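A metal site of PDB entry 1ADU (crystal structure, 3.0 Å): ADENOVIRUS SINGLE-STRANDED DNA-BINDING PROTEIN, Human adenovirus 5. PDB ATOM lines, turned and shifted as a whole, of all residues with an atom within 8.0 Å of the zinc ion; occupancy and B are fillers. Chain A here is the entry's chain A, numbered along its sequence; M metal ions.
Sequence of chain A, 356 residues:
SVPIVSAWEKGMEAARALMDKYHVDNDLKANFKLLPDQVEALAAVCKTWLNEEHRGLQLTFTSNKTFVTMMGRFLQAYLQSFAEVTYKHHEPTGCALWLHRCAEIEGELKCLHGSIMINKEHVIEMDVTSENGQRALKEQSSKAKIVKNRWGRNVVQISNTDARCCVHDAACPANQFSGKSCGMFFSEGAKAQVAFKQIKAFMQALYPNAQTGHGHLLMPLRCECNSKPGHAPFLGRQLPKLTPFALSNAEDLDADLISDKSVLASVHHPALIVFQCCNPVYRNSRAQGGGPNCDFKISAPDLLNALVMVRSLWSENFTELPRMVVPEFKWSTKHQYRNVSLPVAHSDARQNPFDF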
ATOM      1  N   ARG A 222     -18.139  -5.163 -30.096  1.00  0.00           N
ATOM      2  CA  ARG A 222     -16.872  -5.256 -29.384  1.00  0.00           C
ATOM      3  C   ARG A 222     -16.980  -5.226 -27.864  1.00  0.00           C
ATOM      4  O   ARG A 222     -17.704  -4.404 -27.301  1.00  0.00           O
ATOM      5  CB  ARG A 222     -15.919  -4.164 -29.853  1.00  0.00           C
ATOM      6  CG  ARG A 222     -16.363  -2.772 -29.510  1.00  0.00           C
ATOM      7  CD  ARG A 222     -15.325  -1.754 -29.936  1.00  0.00           C
ATOM      8  NE  ARG A 222     -15.574  -1.259 -31.284  1.00  0.00           N
ATOM      9  CZ  ARG A 222     -15.934  -0.008 -31.564  1.00  0.00           C
ATOM     10  NH1 ARG A 222     -16.092   0.872 -30.574  1.00  0.00           N
ATOM     11  NH2 ARG A 222     -16.148   0.362 -32.815  1.00  0.00           N
ATOM     12  N   CYS A 223     -16.285  -6.151 -27.213  1.00  0.00           N
ATOM     13  CA  CYS A 223     -16.268  -6.222 -25.758  1.00  0.00           C
ATOM     14  C   CYS A 223     -15.088  -5.352 -25.310  1.00  0.00           C
ATOM     15  O   CYS A 223     -14.590  -4.535 -26.089  1.00  0.00           O
ATOM     16  CB  CYS A 223     -16.071  -7.661 -25.274  1.00  0.00           C
ATOM     17  SG  CYS A 223     -14.447  -8.382 -25.672  1.00  0.00           S
ATOM     18  N   GLU A 224     -14.630  -5.543 -24.084  1.00  0.00           N
ATOM     19  CA  GLU A 224     -13.505  -4.760 -23.588  1.00  0.00           C
ATOM     20  C   GLU A 224     -12.196  -5.158 -24.272  1.00  0.00           C
ATOM     21  O   GLU A 224     -11.226  -4.397 -24.262  1.00  0.00           O
ATOM     22  CB  GLU A 224     -13.362  -4.925 -22.061  1.00  0.00           C
ATOM     23  CG  GLU A 224     -14.600  -4.525 -21.255  1.00  0.00           C
ATOM     24  CD  GLU A 224     -14.916  -3.036 -21.337  1.00  0.00           C
ATOM     25  OE1 GLU A 224     -14.237  -2.253 -20.649  1.00  0.00           O
ATOM     26  OE2 GLU A 224     -15.859  -2.660 -22.071  1.00  0.00           O
ATOM     27  N   CYS A 225     -12.191  -6.335 -24.891  1.00  0.00           N
ATOM     28  CA  CYS A 225     -11.015  -6.864 -25.570  1.00  0.00           C
ATOM     29  C   CYS A 225     -10.744  -6.258 -26.945  1.00  0.00           C
ATOM     30  O   CYS A 225      -9.705  -5.651 -27.177  1.00  0.00           O
ATOM     31  CB  CYS A 225     -11.124  -8.389 -25.683  1.00  0.00           C
ATOM     32  SG  CYS A 225     -11.315  -9.220 -24.080  1.00  0.00           S
ATOM     33  N   ASN A 226     -11.672  -6.442 -27.871  1.00  0.00           N
ATOM     34  CA  ASN A 226     -11.526  -5.906 -29.206  1.00  0.00           C
ATOM     35  C   ASN A 226     -11.969  -4.464 -29.295  1.00  0.00           C
ATOM     36  O   ASN A 226     -12.744  -4.102 -30.177  1.00  0.00           O
ATOM     37  CB  ASN A 226     -12.242  -6.775 -30.247  1.00  0.00           C
ATOM     38  CG  ASN A 226     -13.671  -7.113 -29.850  1.00  0.00           C
ATOM     39  OD1 ASN A 226     -14.053  -7.023 -28.689  1.00  0.00           O
ATOM     40  ND2 ASN A 226     -14.454  -7.566 -30.824  1.00  0.00           N
ATOM     41  N   SER A 227     -11.434  -3.627 -28.410  1.00  0.00           N
ATOM     42  CA  SER A 227     -11.758  -2.199 -28.357  1.00  0.00           C
ATOM     43  C   SER A 227     -10.540  -1.343 -28.013  1.00  0.00           C
ATOM     44  O   SER A 227      -9.655  -1.827 -27.277  1.00  0.00           O
ATOM     45  CB  SER A 227     -12.870  -1.953 -27.338  1.00  0.00           C
ATOM     46  OG  SER A 227     -12.598  -2.634 -26.131  1.00  0.00           O
ATOM     47  N   PHE A 234      -6.686 -11.746 -31.740  1.00  0.00           N
ATOM     48  CA  PHE A 234      -6.771 -12.866 -30.815  1.00  0.00           C
ATOM     49  C   PHE A 234      -7.580 -13.988 -31.454  1.00  0.00           C
ATOM     50  O   PHE A 234      -8.304 -13.765 -32.432  1.00  0.00           O
ATOM     51  CB  PHE A 234      -7.349 -12.454 -29.452  1.00  0.00           C
ATOM     52  CG  PHE A 234      -8.688 -11.754 -29.536  1.00  0.00           C
ATOM     53  CD1 PHE A 234      -9.869 -12.492 -29.577  1.00  0.00           C
ATOM     54  CD2 PHE A 234      -8.750 -10.373 -29.568  1.00  0.00           C
ATOM     55  CE1 PHE A 234     -11.111 -11.844 -29.639  1.00  0.00           C
ATOM     56  CE2 PHE A 234      -9.989  -9.715 -29.634  1.00  0.00           C
ATOM     57  CZ  PHE A 234     -11.163 -10.453 -29.670  1.00  0.00           C
ATOM     58  N   PRO A 240     -18.792 -10.395 -29.377  1.00  0.00           N
ATOM     59  CA  PRO A 240     -19.293 -10.882 -28.085  1.00  0.00           C
ATOM     60  C   PRO A 240     -20.187 -12.113 -28.273  1.00  0.00           C
ATOM     61  O   PRO A 240     -21.012 -12.147 -29.180  1.00  0.00           O
ATOM     62  CB  PRO A 240     -20.088  -9.691 -27.583  1.00  0.00           C
ATOM     63  CG  PRO A 240     -19.242  -8.542 -28.043  1.00  0.00           C
ATOM     64  CD  PRO A 240     -18.907  -8.932 -29.462  1.00  0.00           C
ATOM     65  N   GLN A 276     -21.883 -11.537 -23.735  1.00  0.00           N
ATOM     66  CA  GLN A 276     -20.718 -11.618 -22.865  1.00  0.00           C
ATOM     67  C   GLN A 276     -19.476 -11.216 -23.658  1.00  0.00           C
ATOM     68  O   GLN A 276     -19.598 -10.538 -24.680  1.00  0.00           O
ATOM     69  CB  GLN A 276     -20.591 -13.050 -22.336  1.00  0.00           C
ATOM     70  CG  GLN A 276     -21.805 -13.491 -21.510  1.00  0.00           C
ATOM     71  CD  GLN A 276     -21.740 -14.936 -21.048  1.00  0.00           C
ATOM     72  OE1 GLN A 276     -21.968 -15.867 -21.823  1.00  0.00           O
ATOM     73  NE2 GLN A 276     -21.444 -15.134 -19.768  1.00  0.00           N
ATOM     74  N   CYS A 277     -18.283 -11.562 -23.170  1.00  0.00           N
ATOM     75  CA  CYS A 277     -17.039 -11.245 -23.876  1.00  0.00           C
ATOM     76  C   CYS A 277     -17.014 -12.091 -25.145  1.00  0.00           C
ATOM     77  O   CYS A 277     -17.742 -13.096 -25.235  1.00  0.00           O
ATOM     78  CB  CYS A 277     -15.831 -11.589 -22.980  1.00  0.00           C
ATOM     79  SG  CYS A 277     -14.176 -11.680 -23.769  1.00  0.00           S
ATOM     80  N   CYS A 278     -16.222 -11.685 -26.136  1.00  0.00           N
ATOM     81  CA  CYS A 278     -16.106 -12.444 -27.382  1.00  0.00           C
ATOM     82  C   CYS A 278     -15.844 -13.905 -27.004  1.00  0.00           C
ATOM     83  O   CYS A 278     -16.529 -14.816 -27.453  1.00  0.00           O
ATOM     84  CB  CYS A 278     -14.946 -11.934 -28.239  1.00  0.00           C
ATOM     85  SG  CYS A 278     -15.077 -10.223 -28.832  1.00  0.00           S
ATOM     86  N   ASN A 279     -14.878 -14.099 -26.107  1.00  0.00           N
ATOM     87  CA  ASN A 279     -14.515 -15.434 -25.639  1.00  0.00           C
ATOM     88  C   ASN A 279     -14.467 -15.456 -24.109  1.00  0.00           C
ATOM     89  O   ASN A 279     -13.481 -15.037 -23.500  1.00  0.00           O
ATOM     90  CB  ASN A 279     -13.147 -15.844 -26.214  1.00  0.00           C
ATOM     91  CG  ASN A 279     -13.174 -16.013 -27.726  1.00  0.00           C
ATOM     92  OD1 ASN A 279     -13.426 -17.107 -28.252  1.00  0.00           O
ATOM     93  ND2 ASN A 279     -12.902 -14.922 -28.448  1.00  0.00           N
ATOM     94  N   PRO A 280     -15.589 -15.856 -23.483  1.00  0.00           N
ATOM     95  CA  PRO A 280     -15.739 -15.942 -22.016  1.00  0.00           C
ATOM     96  C   PRO A 280     -14.806 -16.992 -21.415  1.00  0.00           C
ATOM     97  O   PRO A 280     -14.371 -17.889 -22.171  1.00  0.00           O
ATOM     98  CB  PRO A 280     -17.206 -16.354 -21.852  1.00  0.00           C
ATOM     99  CG  PRO A 280     -17.860 -15.807 -23.069  1.00  0.00           C
ATOM    100  CD  PRO A 280     -16.862 -16.160 -24.144  1.00  0.00           C
ATOM    101  N   PRO A 292      -6.736 -13.114 -24.520  1.00  0.00           N
ATOM    102  CA  PRO A 292      -7.426 -11.983 -23.886  1.00  0.00           C
ATOM    103  C   PRO A 292      -8.799 -12.439 -23.438  1.00  0.00           C
ATOM    104  O   PRO A 292      -9.349 -13.389 -23.986  1.00  0.00           O
ATOM    105  CB  PRO A 292      -7.552 -10.899 -24.944  1.00  0.00           C
ATOM    106  CG  PRO A 292      -6.324 -11.181 -25.795  1.00  0.00           C
ATOM    107  CD  PRO A 292      -6.232 -12.723 -25.845  1.00  0.00           C
ATOM    108  N   ASN A 293      -9.338 -11.767 -22.421  1.00  0.00           N
ATOM    109  CA  ASN A 293     -10.652 -12.070 -21.876  1.00  0.00           C
ATOM    110  C   ASN A 293     -11.049 -10.843 -21.073  1.00  0.00           C
ATOM    111  O   ASN A 293     -10.198 -10.000 -20.767  1.00  0.00           O
ATOM    112  CB  ASN A 293     -10.568 -13.309 -20.957  1.00  0.00           C
ATOM    113  CG  ASN A 293     -11.885 -13.614 -20.271  1.00  0.00           C
ATOM    114  OD1 ASN A 293     -12.189 -13.058 -19.213  1.00  0.00           O
ATOM    115  ND2 ASN A 293     -12.682 -14.483 -20.874  1.00  0.00           N
ATOM    116  N   CYS A 294     -12.334 -10.696 -20.770  1.00  0.00           N
ATOM    117  CA  CYS A 294     -12.800  -9.556 -20.002  1.00  0.00           C
ATOM    118  C   CYS A 294     -14.128  -9.866 -19.335  1.00  0.00           C
ATOM    119  O   CYS A 294     -14.753 -10.885 -19.636  1.00  0.00           O
ATOM    120  CB  CYS A 294     -12.935  -8.317 -20.902  1.00  0.00           C
ATOM    121  SG  CYS A 294     -14.374  -8.299 -22.005  1.00  0.00           S
ATOM    122  N   ASP A 295     -14.561  -8.976 -18.444  1.00  0.00           N
ATOM    123  CA  ASP A 295     -15.815  -9.144 -17.718  1.00  0.00           C
ATOM    124  C   ASP A 295     -16.936  -8.279 -18.320  1.00  0.00           C
ATOM    125  O   ASP A 295     -17.533  -7.440 -17.644  1.00  0.00           O
ATOM    126  CB  ASP A 295     -15.618  -8.836 -16.244  1.00  0.00           C
ATOM    127  CG  ASP A 295     -14.615  -9.761 -15.576  1.00  0.00           C
ATOM    128  OD1 ASP A 295     -14.854 -10.985 -15.563  1.00  0.00           O
ATOM    129  OD2 ASP A 295     -13.582  -9.253 -15.091  1.00  0.00           O
ATOM    130  N   PHE A 296     -17.202  -8.510 -19.599  1.00  0.00           N
ATOM    131  CA  PHE A 296     -18.233  -7.794 -20.318  1.00  0.00           C
ATOM    132  C   PHE A 296     -19.475  -8.667 -20.199  1.00  0.00           C
ATOM    133  O   PHE A 296     -19.442  -9.857 -20.532  1.00  0.00           O
ATOM    134  CB  PHE A 296     -17.824  -7.629 -21.773  1.00  0.00           C
ATOM    135  CG  PHE A 296     -18.785  -6.828 -22.610  1.00  0.00           C
ATOM    136  CD1 PHE A 296     -19.913  -7.421 -23.165  1.00  0.00           C
ATOM    137  CD2 PHE A 296     -18.531  -5.483 -22.893  1.00  0.00           C
ATOM    138  CE1 PHE A 296     -20.773  -6.695 -24.003  1.00  0.00           C
ATOM    139  CE2 PHE A 296     -19.388  -4.752 -23.718  1.00  0.00           C
ATOM    140  CZ  PHE A 296     -20.505  -5.358 -24.270  1.00  0.00           C
HETATM  141 ZN    ZN M   1     -13.588  -9.478 -23.815  1.00  0.00          ZN
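SG of Cys 277 sits close to N of Asn 279 (3.4 Å). The backbone NH of Cys 223 is in hydrogen-bond range of the side-chain amide oxygen of Asn 226 (2.8 Å). The backbone carbonyl oxygen (O) of Asn 293 sits close to the side-chain sulfur (SG) of Cys 225, 3.6 Å away. O of Asn 279 lies within hydrogen-bond range of ND2 of Asn 293 (2.8 Å). O of Cys 223 sits at hydrogen-bond distance from OG of Ser 227, at 2.8 Å. N of Phe 296 lies close to SG of Cys 294 (3.7 Å). The backbone NH (N) of Cys 277 sits at hydrogen-bond distance from the backbone carbonyl oxygen (O) of Phe 296 (3.3 Å). The backbone NH of Glu 224 lies close to the side-chain sulfur of Cys 294, 3.5 Å away.
The zinc ion is bound by the side-chain sulfur (SG) of Cys 277, the side-chain sulfur (SG) of Cys 294, the side-chain sulfur (SG) of Cys 225 and the side-chain sulfur (SG) of Cys 223.
C of Asn 293 touches the zinc ion, at 3.98 Å. Five residues have an atom within 4 Å of the zinc ion: Cys 223, Cys 225, Cys 277, Asn 293 and Cys 294.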
